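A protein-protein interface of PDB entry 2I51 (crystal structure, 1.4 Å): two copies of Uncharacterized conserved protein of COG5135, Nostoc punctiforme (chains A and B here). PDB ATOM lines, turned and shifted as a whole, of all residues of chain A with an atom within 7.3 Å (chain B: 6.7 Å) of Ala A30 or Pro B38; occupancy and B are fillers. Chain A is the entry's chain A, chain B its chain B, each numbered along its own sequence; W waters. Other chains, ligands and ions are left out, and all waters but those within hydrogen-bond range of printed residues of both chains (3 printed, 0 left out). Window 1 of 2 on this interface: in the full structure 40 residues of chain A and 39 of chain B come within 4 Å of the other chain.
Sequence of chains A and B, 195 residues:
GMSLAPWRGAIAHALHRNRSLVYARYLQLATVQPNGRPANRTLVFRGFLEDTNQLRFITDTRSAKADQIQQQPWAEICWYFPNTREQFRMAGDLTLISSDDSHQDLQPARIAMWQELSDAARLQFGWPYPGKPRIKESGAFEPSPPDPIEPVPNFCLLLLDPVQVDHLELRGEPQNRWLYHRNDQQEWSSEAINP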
ATOM      1  N   LEU A  27     -26.590  -0.670 -22.696  1.00  0.00           N
ATOM      2  CA  LEU A  27     -26.388   0.632 -23.303  1.00  0.00           C
ATOM      3  C   LEU A  27     -26.389   1.689 -22.208  1.00  0.00           C
ATOM      4  O   LEU A  27     -26.813   1.437 -21.062  1.00  0.00           O
ATOM      5  CB  LEU A  27     -27.424   0.901 -24.392  1.00  0.00           C
ATOM      6  CG  LEU A  27     -28.902   0.841 -24.011  1.00  0.00           C
ATOM      7  CD1 LEU A  27     -29.284   2.088 -23.181  1.00  0.00           C
ATOM      8  CD2 LEU A  27     -29.811   0.722 -25.305  1.00  0.00           C
ATOM      9  N   GLN A  28     -25.941   2.889 -22.518  1.00  0.00           N
ATOM     10  CA  GLN A  28     -25.808   3.956 -21.533  1.00  0.00           C
ATOM     11  C   GLN A  28     -26.832   5.045 -21.742  1.00  0.00           C
ATOM     12  O   GLN A  28     -26.898   5.628 -22.857  1.00  0.00           O
ATOM     13  CB  GLN A  28     -24.377   4.510 -21.527  1.00  0.00           C
ATOM     14  CG  GLN A  28     -23.350   3.527 -20.985  1.00  0.00           C
ATOM     15  CD  GLN A  28     -23.079   2.342 -21.845  1.00  0.00           C
ATOM     16  OE1 GLN A  28     -22.985   2.466 -23.082  1.00  0.00           O
ATOM     17  NE2 GLN A  28     -22.991   1.144 -21.225  1.00  0.00           N
ATOM     18  N   LEU A  29     -27.592   5.347 -20.694  1.00  0.00           N
ATOM     19  CA  LEU A  29     -28.641   6.360 -20.803  1.00  0.00           C
ATOM     20  C   LEU A  29     -28.206   7.596 -20.044  1.00  0.00           C
ATOM     21  O   LEU A  29     -27.993   7.583 -18.807  1.00  0.00           O
ATOM     22  CB  LEU A  29     -29.920   5.854 -20.146  1.00  0.00           C
ATOM     23  CG  LEU A  29     -31.048   6.906 -19.993  1.00  0.00           C
ATOM     24  CD1 LEU A  29     -31.736   6.971 -21.303  1.00  0.00           C
ATOM     25  CD2 LEU A  29     -31.995   6.558 -18.817  1.00  0.00           C
ATOM     26  N   ALA A  30     -28.121   8.721 -20.773  1.00  0.00           N
ATOM     27  CA  ALA A  30     -27.791   9.998 -20.178  1.00  0.00           C
ATOM     28  C   ALA A  30     -29.052  10.820 -19.982  1.00  0.00           C
ATOM     29  O   ALA A  30     -29.859  10.971 -20.885  1.00  0.00           O
ATOM     30  CB  ALA A  30     -26.805  10.792 -21.106  1.00  0.00           C
ATOM     31  N   THR A  31     -29.162  11.409 -18.801  1.00  0.00           N
ATOM     32  CA  THR A  31     -30.216  12.325 -18.454  1.00  0.00           C
ATOM     33  C   THR A  31     -29.587  13.597 -17.884  1.00  0.00           C
ATOM     34  O   THR A  31     -28.350  13.694 -17.773  1.00  0.00           O
ATOM     35  CB  THR A  31     -31.128  11.699 -17.343  1.00  0.00           C
ATOM     36  OG1 THR A  31     -30.297  11.264 -16.229  1.00  0.00           O
ATOM     37  CG2 THR A  31     -31.973  10.564 -17.860  1.00  0.00           C
ATOM     38  N   VAL A  32     -30.419  14.603 -17.577  1.00  0.00           N
ATOM     39  CA  VAL A  32     -29.945  15.828 -16.942  1.00  0.00           C
ATOM     40  C   VAL A  32     -30.603  15.926 -15.573  1.00  0.00           C
ATOM     41  O   VAL A  32     -31.828  15.650 -15.400  1.00  0.00           O
ATOM     42  CB  VAL A  32     -30.202  17.101 -17.809  1.00  0.00           C
ATOM     43  CG1 VAL A  32     -29.548  18.365 -17.194  1.00  0.00           C
ATOM     44  CG2 VAL A  32     -29.622  16.949 -19.168  1.00  0.00           C
ATOM     45  N   PRO A  38     -25.188  16.527 -16.075  1.00  0.00           N
ATOM     46  CA  PRO A  38     -25.571  15.262 -16.707  1.00  0.00           C
ATOM     47  C   PRO A  38     -25.441  14.113 -15.720  1.00  0.00           C
ATOM     48  O   PRO A  38     -24.745  14.195 -14.699  1.00  0.00           O
ATOM     49  CB  PRO A  38     -24.541  15.124 -17.816  1.00  0.00           C
ATOM     50  CG  PRO A  38     -23.356  15.812 -17.264  1.00  0.00           C
ATOM     51  CD  PRO A  38     -23.843  16.965 -16.492  1.00  0.00           C
ATOM     52  N   ALA A  39     -26.112  13.022 -16.063  1.00  0.00           N
ATOM     53  CA  ALA A  39     -26.018  11.730 -15.358  1.00  0.00           C
ATOM     54  C   ALA A  39     -26.018  10.665 -16.425  1.00  0.00           C
ATOM     55  O   ALA A  39     -26.606  10.836 -17.480  1.00  0.00           O
ATOM     56  CB  ALA A  39     -27.187  11.512 -14.362  1.00  0.00           C
ATOM     57  N   ASN A  40     -25.329   9.583 -16.164  1.00  0.00           N
ATOM     58  CA  ASN A  40     -25.108   8.561 -17.181  1.00  0.00           C
ATOM     59  C   ASN A  40     -24.958   7.206 -16.509  1.00  0.00           C
ATOM     60  O   ASN A  40     -24.127   7.062 -15.635  1.00  0.00           O
ATOM     61  CB  ASN A  40     -23.833   8.932 -17.927  1.00  0.00           C
ATOM     62  CG  ASN A  40     -23.706   8.283 -19.305  1.00  0.00           C
ATOM     63  OD1 ASN A  40     -24.641   7.656 -19.812  1.00  0.00           O
ATOM     64  ND2 ASN A  40     -22.500   8.484 -19.941  1.00  0.00           N
ATOM     65  N   ARG A  41     -25.739   6.219 -16.948  1.00  0.00           N
ATOM     66  CA  ARG A  41     -25.635   4.858 -16.376  1.00  0.00           C
ATOM     67  C   ARG A  41     -26.056   3.822 -17.362  1.00  0.00           C
ATOM     68  O   ARG A  41     -26.825   4.094 -18.282  1.00  0.00           O
ATOM     69  CB  ARG A  41     -26.451   4.725 -15.098  1.00  0.00           C
ATOM     70  CG  ARG A  41     -27.909   4.516 -15.281  1.00  0.00           C
ATOM     71  CD  ARG A  41     -28.665   5.737 -15.769  1.00  0.00           C
ATOM     72  NE  ARG A  41     -28.754   6.814 -14.803  1.00  0.00           N
ATOM     73  CZ  ARG A  41     -29.128   8.072 -15.027  1.00  0.00           C
ATOM     74  NH1 ARG A  41     -29.248   8.570 -16.271  1.00  0.00           N
ATOM     75  NH2 ARG A  41     -29.315   8.860 -14.005  1.00  0.00           N
ATOM     76  N   LEU A  43     -28.052   0.566 -18.691  1.00  0.00           N
ATOM     77  CA  LEU A  43     -29.282  -0.174 -18.557  1.00  0.00           C
ATOM     78  C   LEU A  43     -29.260  -1.336 -19.517  1.00  0.00           C
ATOM     79  O   LEU A  43     -28.516  -1.336 -20.485  1.00  0.00           O
ATOM     80  CB  LEU A  43     -30.501   0.657 -18.953  1.00  0.00           C
ATOM     81  CG  LEU A  43     -30.616   2.043 -18.343  1.00  0.00           C
ATOM     82  CD1 LEU A  43     -31.807   2.814 -18.999  1.00  0.00           C
ATOM     83  CD2 LEU A  43     -30.759   1.854 -16.905  1.00  0.00           C
ATOM     84  N   GLN A  68     -35.190  12.426 -11.922  1.00  0.00           N
ATOM     85  CA  GLN A  68     -34.567  13.224 -12.984  1.00  0.00           C
ATOM     86  C   GLN A  68     -35.464  13.187 -14.224  1.00  0.00           C
ATOM     87  O   GLN A  68     -35.670  14.207 -14.874  1.00  0.00           O
ATOM     88  CB  GLN A  68     -33.182  12.692 -13.366  1.00  0.00           C
ATOM     89  CG  GLN A  68     -32.125  12.744 -12.216  1.00  0.00           C
ATOM     90  CD  GLN A  68     -30.902  11.914 -12.482  1.00  0.00           C
ATOM     91  OE1 GLN A  68     -30.682  11.422 -13.591  1.00  0.00           O
ATOM     92  NE2 GLN A  68     -30.078  11.746 -11.449  1.00  0.00           N
ATOM     93  N   GLN A  72     -37.234  16.176 -16.350  1.00  0.00           N
ATOM     94  CA  GLN A  72     -36.769  16.431 -17.713  1.00  0.00           C
ATOM     95  C   GLN A  72     -36.751  15.095 -18.442  1.00  0.00           C
ATOM     96  O   GLN A  72     -35.804  14.328 -18.321  1.00  0.00           O
ATOM     97  CB  GLN A  72     -35.405  17.095 -17.694  1.00  0.00           C
ATOM     98  CG  GLN A  72     -34.587  17.138 -19.008  1.00  0.00           C
ATOM     99  CD  GLN A  72     -35.239  17.843 -20.140  1.00  0.00           C
ATOM    100  OE1 GLN A  72     -36.202  17.361 -20.721  1.00  0.00           O
ATOM    101  NE2 GLN A  72     -34.705  19.015 -20.488  1.00  0.00           N
ATOM    102  N   PRO A  73     -37.830  14.803 -19.157  1.00  0.00           N
ATOM    103  CA  PRO A  73     -37.923  13.502 -19.797  1.00  0.00           C
ATOM    104  C   PRO A  73     -36.948  13.322 -21.034  1.00  0.00           C
ATOM    105  O   PRO A  73     -36.849  12.274 -21.602  1.00  0.00           O
ATOM    106  CB  PRO A  73     -39.450  13.366 -20.049  1.00  0.00           C
ATOM    107  CG  PRO A  73     -39.974  14.748 -20.136  1.00  0.00           C
ATOM    108  CD  PRO A  73     -39.053  15.620 -19.305  1.00  0.00           C
ATOM    109  N   TRP A  74     -36.240  14.340 -21.482  1.00  0.00           N
ATOM    110  CA  TRP A  74     -35.433  14.106 -22.680  1.00  0.00           C
ATOM    111  C   TRP A  74     -34.112  13.399 -22.323  1.00  0.00           C
ATOM    112  O   TRP A  74     -33.422  13.859 -21.407  1.00  0.00           O
ATOM    113  CB  TRP A  74     -35.163  15.405 -23.309  1.00  0.00           C
ATOM    114  CG  TRP A  74     -34.481  15.220 -24.596  1.00  0.00           C
ATOM    115  CD1 TRP A  74     -33.155  14.983 -24.786  1.00  0.00           C
ATOM    116  CD2 TRP A  74     -35.078  15.258 -25.883  1.00  0.00           C
ATOM    117  NE1 TRP A  74     -32.887  14.863 -26.104  1.00  0.00           N
ATOM    118  CE2 TRP A  74     -34.048  15.074 -26.816  1.00  0.00           C
ATOM    119  CE3 TRP A  74     -36.390  15.446 -26.344  1.00  0.00           C
ATOM    120  CZ2 TRP A  74     -34.276  15.065 -28.191  1.00  0.00           C
ATOM    121  CZ3 TRP A  74     -36.606  15.443 -27.720  1.00  0.00           C
ATOM    122  CH2 TRP A  74     -35.568  15.274 -28.615  1.00  0.00           C
ATOM    123  N   ALA A  75     -33.787  12.300 -23.021  1.00  0.00           N
ATOM    124  CA  ALA A  75     -32.562  11.527 -22.722  1.00  0.00           C
ATOM    125  C   ALA A  75     -31.801  11.251 -24.019  1.00  0.00           C
ATOM    126  O   ALA A  75     -32.369  11.360 -25.109  1.00  0.00           O
ATOM    127  CB  ALA A  75     -32.877  10.250 -22.012  1.00  0.00           C
ATOM    128  N   GLU A  76     -30.532  10.868 -23.881  1.00  0.00           N
ATOM    129  CA  GLU A  76     -29.793  10.403 -25.022  1.00  0.00           C
ATOM    130  C   GLU A  76     -29.074   9.116 -24.640  1.00  0.00           C
ATOM    131  O   GLU A  76     -28.337   9.071 -23.629  1.00  0.00           O
ATOM    132  CB  GLU A  76     -28.743  11.416 -25.471  1.00  0.00           C
ATOM    133  CG  GLU A  76     -28.069  10.989 -26.787  1.00  0.00           C
ATOM    134  CD  GLU A  76     -27.354  12.148 -27.471  1.00  0.00           C
ATOM    135  OE1 GLU A  76     -28.038  13.154 -27.863  1.00  0.00           O
ATOM    136  OE2 GLU A  76     -26.125  12.108 -27.645  1.00  0.00           O
ATOM    137  N   ILE A  77     -29.361   8.058 -25.390  1.00  0.00           N
ATOM    138  CA  ILE A  77     -28.628   6.834 -25.165  1.00  0.00           C
ATOM    139  C   ILE A  77     -27.420   6.775 -26.101  1.00  0.00           C
ATOM    140  O   ILE A  77     -27.402   7.350 -27.196  1.00  0.00           O
ATOM    141  CB  ILE A  77     -29.504   5.597 -25.274  1.00  0.00           C
ATOM    142  CG1 ILE A  77     -30.126   5.529 -26.678  1.00  0.00           C
ATOM    143  CG2 ILE A  77     -30.525   5.551 -24.105  1.00  0.00           C
ATOM    144  CD1 ILE A  77     -30.775   4.170 -26.986  1.00  0.00           C
ATOM    145  N   CYS A  78     -26.366   6.119 -25.623  1.00  0.00           N
ATOM    146  CA  CYS A  78     -25.236   5.762 -26.443  1.00  0.00           C
ATOM    147  C   CYS A  78     -25.110   4.278 -26.310  1.00  0.00           C
ATOM    148  O   CYS A  78     -25.066   3.730 -25.214  1.00  0.00           O
ATOM    149  CB  CYS A  78     -23.988   6.466 -25.984  1.00  0.00           C
ATOM    150  SG  CYS A  78     -22.578   6.128 -27.048  1.00  0.00           S
ATOM    151  N   ARG A  89     -26.318   6.553 -31.269  1.00  0.00           N
ATOM    152  CA  ARG A  89     -26.728   7.562 -30.295  1.00  0.00           C
ATOM    153  C   ARG A  89     -28.165   7.887 -30.613  1.00  0.00           C
ATOM    154  O   ARG A  89     -28.484   8.098 -31.782  1.00  0.00           O
ATOM    155  CB  ARG A  89     -25.852   8.814 -30.385  1.00  0.00           C
ATOM    156  CG  ARG A  89     -24.444   8.550 -29.972  1.00  0.00           C
ATOM    157  CD  ARG A  89     -23.523   9.715 -30.346  1.00  0.00           C
ATOM    158  NE  ARG A  89     -23.931  10.942 -29.645  1.00  0.00           N
ATOM    159  CZ  ARG A  89     -23.334  12.128 -29.768  1.00  0.00           C
ATOM    160  NH1 ARG A  89     -22.410  12.244 -30.651  1.00  0.00           N
ATOM    161  NH2 ARG A  89     -23.748  13.181 -29.048  1.00  0.00           N
ATOM    162  N   MET A  90     -29.045   7.842 -29.645  1.00  0.00           N
ATOM    163  CA  MET A  90     -30.463   8.007 -29.894  1.00  0.00           C
ATOM    164  C   MET A  90     -31.021   8.975 -28.838  1.00  0.00           C
ATOM    165  O   MET A  90     -30.919   8.711 -27.645  1.00  0.00           O
ATOM    166  CB  MET A  90     -31.177   6.629 -29.908  1.00  0.00           C
ATOM    167  CG  MET A  90     -30.350   5.494 -30.579  1.00  0.00           C
ATOM    168  SD  MET A  90     -31.079   3.690 -30.375  1.00  0.00           S
ATOM    169  CE  MET A  90     -32.196   3.647 -31.959  1.00  0.00           C
ATOM    170  N   ALA A  91     -31.616  10.062 -29.299  1.00  0.00           N
ATOM    171  CA  ALA A  91     -32.117  11.096 -28.412  1.00  0.00           C
ATOM    172  C   ALA A  91     -33.607  11.228 -28.583  1.00  0.00           C
ATOM    173  O   ALA A  91     -34.099  11.167 -29.692  1.00  0.00           O
ATOM    174  CB  ALA A  91     -31.489  12.392 -28.736  1.00  0.00           C
ATOM    175  N   GLY A  92     -34.327  11.403 -27.482  1.00  0.00           N
ATOM    176  CA  GLY A  92     -35.758  11.617 -27.559  1.00  0.00           C
ATOM    177  C   GLY A  92     -36.389  11.601 -26.191  1.00  0.00           C
ATOM    178  O   GLY A  92     -35.710  11.676 -25.170  1.00  0.00           O
ATOM    179  N   LEU A  94     -38.521  10.408 -22.979  1.00  0.00           N
ATOM    180  CA  LEU A  94     -38.808   9.292 -22.130  1.00  0.00           C
ATOM    181  C   LEU A  94     -40.230   9.316 -21.621  1.00  0.00           C
ATOM    182  O   LEU A  94     -40.770  10.341 -21.320  1.00  0.00           O
ATOM    183  CB  LEU A  94     -37.874   9.267 -20.921  1.00  0.00           C
ATOM    184  CG  LEU A  94     -36.386   9.031 -21.258  1.00  0.00           C
ATOM    185  CD1 LEU A  94     -35.472   9.304 -20.028  1.00  0.00           C
ATOM    186  CD2 LEU A  94     -36.145   7.645 -21.830  1.00  0.00           C
ATOM    187  N   LEU B  29     -19.156   9.327 -22.418  1.00  0.00           N
ATOM    188  CA  LEU B  29     -19.041  10.646 -21.784  1.00  0.00           C
ATOM    189  C   LEU B  29     -20.335  11.414 -22.064  1.00  0.00           C
ATOM    190  O   LEU B  29     -20.705  11.695 -23.220  1.00  0.00           O
ATOM    191  CB  LEU B  29     -17.893  11.438 -22.444  1.00  0.00           C
ATOM    192  CG  LEU B  29     -17.896  12.956 -22.020  1.00  0.00           C
ATOM    193  CD1 LEU B  29     -17.356  12.993 -20.619  1.00  0.00           C
ATOM    194  CD2 LEU B  29     -17.111  13.876 -22.983  1.00  0.00           C
ATOM    195  N   ALA B  30     -21.053  11.760 -21.018  1.00  0.00           N
ATOM    196  CA  ALA B  30     -22.246  12.582 -21.089  1.00  0.00           C
ATOM    197  C   ALA B  30     -21.956  14.011 -20.706  1.00  0.00           C
ATOM    198  O   ALA B  30     -21.344  14.297 -19.677  1.00  0.00           O
ATOM    199  CB  ALA B  30     -23.320  12.019 -20.122  1.00  0.00           C
ATOM    200  N   THR B  31     -22.457  14.915 -21.561  1.00  0.00           N
ATOM    201  CA  THR B  31     -22.394  16.326 -21.355  1.00  0.00           C
ATOM    202  C   THR B  31     -23.834  16.903 -21.431  1.00  0.00           C
ATOM    203  O   THR B  31     -24.776  16.194 -21.740  1.00  0.00           O
ATOM    204  CB  THR B  31     -21.517  16.992 -22.393  1.00  0.00           C
ATOM    205  OG1 THR B  31     -21.961  16.599 -23.693  1.00  0.00           O
ATOM    206  CG2 THR B  31     -20.051  16.592 -22.224  1.00  0.00           C
ATOM    207  N   VAL B  32     -23.971  18.195 -21.186  1.00  0.00           N
ATOM    208  CA  VAL B  32     -25.248  18.876 -21.377  1.00  0.00           C
ATOM    209  C   VAL B  32     -25.034  19.920 -22.452  1.00  0.00           C
ATOM    210  O   VAL B  32     -23.990  20.625 -22.485  1.00  0.00           O
ATOM    211  CB  VAL B  32     -25.790  19.404 -20.051  1.00  0.00           C
ATOM    212  CG1 VAL B  32     -27.164  20.152 -20.238  1.00  0.00           C
ATOM    213  CG2 VAL B  32     -25.974  18.267 -19.083  1.00  0.00           C
ATOM    214  N   GLN B  33     -26.010  20.018 -23.340  1.00  0.00           N
ATOM    215  CA  GLN B  33     -26.025  21.020 -24.395  1.00  0.00           C
ATOM    216  C   GLN B  33     -26.561  22.357 -23.874  1.00  0.00           C
ATOM    217  O   GLN B  33     -27.277  22.418 -22.864  1.00  0.00           O
ATOM    218  CB  GLN B  33     -26.890  20.496 -25.554  1.00  0.00           C
ATOM    219  CG  GLN B  33     -26.499  19.114 -26.098  1.00  0.00           C
ATOM    220  CD  GLN B  33     -27.476  18.652 -27.130  1.00  0.00           C
ATOM    221  OE1 GLN B  33     -27.694  19.336 -28.141  1.00  0.00           O
ATOM    222  NE2 GLN B  33     -28.137  17.561 -26.871  1.00  0.00           N
ATOM    223  N   ASN B  35     -29.031  23.972 -24.913  1.00  0.00           N
ATOM    224  CA  ASN B  35     -30.468  23.893 -24.748  1.00  0.00           C
ATOM    225  C   ASN B  35     -30.957  23.035 -23.581  1.00  0.00           C
ATOM    226  O   ASN B  35     -32.155  22.851 -23.422  1.00  0.00           O
ATOM    227  CB  ASN B  35     -31.134  23.438 -26.032  1.00  0.00           C
ATOM    228  CG  ASN B  35     -30.795  22.005 -26.377  1.00  0.00           C
ATOM    229  OD1 ASN B  35     -30.247  21.246 -25.545  1.00  0.00           O
ATOM    230  ND2 ASN B  35     -31.118  21.613 -27.604  1.00  0.00           N
ATOM    231  N   GLY B  36     -30.035  22.518 -22.768  1.00  0.00           N
ATOM    232  CA  GLY B  36     -30.400  21.783 -21.567  1.00  0.00           C
ATOM    233  C   GLY B  36     -30.530  20.289 -21.727  1.00  0.00           C
ATOM    234  O   GLY B  36     -30.779  19.607 -20.760  1.00  0.00           O
ATOM    235  N   ARG B  37     -30.385  19.792 -22.945  1.00  0.00           N
ATOM    236  CA  ARG B  37     -30.543  18.374 -23.210  1.00  0.00           C
ATOM    237  C   ARG B  37     -29.225  17.666 -23.093  1.00  0.00           C
ATOM    238  O   ARG B  37     -28.190  18.228 -23.402  1.00  0.00           O
ATOM    239  CB  ARG B  37     -31.101  18.210 -24.613  1.00  0.00           C
ATOM    240  CG  ARG B  37     -32.540  18.658 -24.715  1.00  0.00           C
ATOM    241  CD  ARG B  37     -33.033  18.562 -26.120  1.00  0.00           C
ATOM    242  NE  ARG B  37     -34.477  18.829 -26.184  1.00  0.00           N
ATOM    243  CZ  ARG B  37     -35.181  18.870 -27.310  1.00  0.00           C
ATOM    244  NH1 ARG B  37     -34.587  18.697 -28.481  1.00  0.00           N
ATOM    245  NH2 ARG B  37     -36.484  19.119 -27.263  1.00  0.00           N
ATOM    246  N   PRO B  38     -29.256  16.418 -22.630  1.00  0.00           N
ATOM    247  CA  PRO B  38     -28.017  15.642 -22.534  1.00  0.00           C
ATOM    248  C   PRO B  38     -27.461  15.239 -23.896  1.00  0.00           C
ATOM    249  O   PRO B  38     -28.199  15.237 -24.889  1.00  0.00           O
ATOM    250  CB  PRO B  38     -28.432  14.374 -21.795  1.00  0.00           C
ATOM    251  CG  PRO B  38     -29.864  14.248 -22.112  1.00  0.00           C
ATOM    252  CD  PRO B  38     -30.434  15.628 -22.227  1.00  0.00           C
ATOM    253  N   ALA B  39     -26.180  14.861 -23.915  1.00  0.00           N
ATOM    254  CA  ALA B  39     -25.534  14.296 -25.085  1.00  0.00           C
ATOM    255  C   ALA B  39     -24.619  13.234 -24.537  1.00  0.00           C
ATOM    256  O   ALA B  39     -24.150  13.362 -23.415  1.00  0.00           O
ATOM    257  CB  ALA B  39     -24.759  15.339 -25.811  1.00  0.00           C
ATOM    258  N   ASN B  40     -24.388  12.163 -25.291  1.00  0.00           N
ATOM    259  CA  ASN B  40     -23.672  10.979 -24.791  1.00  0.00           C
ATOM    260  C   ASN B  40     -22.966  10.281 -25.939  1.00  0.00           C
ATOM    261  O   ASN B  40     -23.594  10.013 -26.945  1.00  0.00           O
ATOM    262  CB  ASN B  40     -24.714  10.009 -24.230  1.00  0.00           C
ATOM    263  CG  ASN B  40     -24.153   9.000 -23.238  1.00  0.00           C
ATOM    264  OD1 ASN B  40     -23.005   9.083 -22.840  1.00  0.00           O
ATOM    265  ND2 ASN B  40     -25.032   8.108 -22.735  1.00  0.00           N
ATOM    266  N   GLN B  68     -19.990  22.336 -26.334  1.00  0.00           N
ATOM    267  CA  GLN B  68     -20.787  21.974 -25.167  1.00  0.00           C
ATOM    268  C   GLN B  68     -19.953  22.119 -23.916  1.00  0.00           C
ATOM    269  O   GLN B  68     -20.402  22.642 -22.926  1.00  0.00           O
ATOM    270  CB  GLN B  68     -21.308  20.552 -25.272  1.00  0.00           C
ATOM    271  CG  GLN B  68     -22.259  20.357 -26.419  1.00  0.00           C
ATOM    272  CD  GLN B  68     -22.561  18.896 -26.725  1.00  0.00           C
ATOM    273  OE1 GLN B  68     -22.197  17.977 -25.968  1.00  0.00           O
ATOM    274  NE2 GLN B  68     -23.229  18.667 -27.881  1.00  0.00           N
HETATM  275  O   HOH W   1     -30.050  14.827 -26.694  1.00  0.00           O
HETATM  276  O   HOH W   2     -23.669  16.118 -29.250  1.00  0.00           O
HETATM  277  O   HOH W   3     -36.283  18.474 -23.588  1.00  0.00           O
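The backbone carbonyl oxygen (O) of Gln A28 sits at hydrogen-bond distance from the side-chain amide nitrogen (ND2) of Asn B40, 3.1 Å away. The side-chain amide oxygen of Asn A40 is in hydrogen-bond range of the side-chain amide nitrogen of Asn B40 (3.0 Å). The side-chain carboxylate (OE2) of Glu A76 sits at hydrogen-bond distance from the backbone NH (N) of Asn B40 (2.9 Å). NE of Arg A89 is in hydrogen-bond range of O of Asn B40 (2.9 Å).
The backbone NH of Ala A30 lies within hydrogen-bond range of the backbone carbonyl oxygen of Glu A76, at 2.9 Å. The side-chain amide oxygen of Gln A72 is in hydrogen-bond range of the backbone NH of Trp A74, at 3.1 Å. The backbone NH of Ala A75 lies within hydrogen-bond range of the backbone carbonyl oxygen of Gly A92 (3.0 Å). OE2 of Glu A76 is in salt-bridge range of NH2 of Arg A89. The side-chain amide nitrogen of Gln B33 sits at hydrogen-bond distance from the backbone carbonyl oxygen of Pro B38, 3.1 Å away. The side-chain amide oxygen (OD1) of Asn B35 is in hydrogen-bond range of the backbone NH (N) of Arg B37, at 3.0 Å.
CB of Ala A30 touches CB of Ala B30, at 3.8 Å. Ala A30 touches Pro B38 (O to CG, 3.5 Å). Asn B40 touches Ala A30. CG2 of Val A32 touches CG2 of Val B32, 3.9 Å away. Val A32 touches Gly B36. CD of Pro B38 touches CG2 of Val A32 (3.4 Å). Val B32 touches Pro A38 (CG2 to N, 3.6 Å). Asn A40 touches Ala B30 (ND2 to CB, 3.6 Å). O of Trp A74 touches CD of Pro B38 (3.6 Å). Cys A78 touches Asn B40 (CB to O, 3.7 Å).
Of chain B, only Ala B30, Pro B38 and Asn B40 come within 4 Å of Ala A30. Printed residues of chain B within 4 Å of Trp A74: Arg B37 (3.6 Å) and Pro B38 (3.6 Å). Of the printed residues of chain B, Cys A78 touches Asn B40. Of the printed residues of chain B, Arg A89 touches Asn B40. Of the printed residues of chain A, Val B32 touches Val A32 (3.9 Å) and Pro A38 (3.6 Å). Of the printed residues of chain A, Pro B38 touches Ala A30, Val A32, Trp A74, Ala A75 and Glu A76.
Of the 24 printed residues of chain A, 11 touch a printed residue of chain B. Hydrophobic or aromatic side chains of chain A that line the printed part of chain B: Ala A30, Val A32, Pro A38 and Trp A74. Hydrophobic or aromatic side chains of chain B that line the printed part of chain A: Ala B30, Val B32, Pro B38 and Ala B39. Among the printed residues, no Asp or Glu carboxylate lies within 4 Å of a Lys or Arg side-chain nitrogen of the other chain.
Ala A30 touches its own counterpart, Ala B30. Ala A30 touches Pro B38, and with the chains exchanged Pro A38 touches Ala B30. Ala A30 touches Asn B40, and with the chains exchanged Asn A40 touches Ala B30. Asn A40 touches its own counterpart, Asn B40. Of the 20 pairs that touch across the chains among the printed residues, 9 have their exchanged pair printed and touching as well.
Water W1 lies within hydrogen-bond range of O of Pro B38 (2.6 Å), OE1 of Glu A76 (2.9 Å), NE1 of Trp A74 (2.9 Å) and NE2 of Gln B33 (3.3 Å). Water W2 lies within hydrogen-bond range of the side-chain amide nitrogen (NE2) of Gln B68 (2.9 Å) and the guanidinium group (NH2) of Arg A89 (2.9 Å). Water W3 lies within hydrogen-bond range of the side-chain amide oxygen of Gln A72 (3.1 Å) and the guanidinium group of Arg B37 (3.2 Å).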
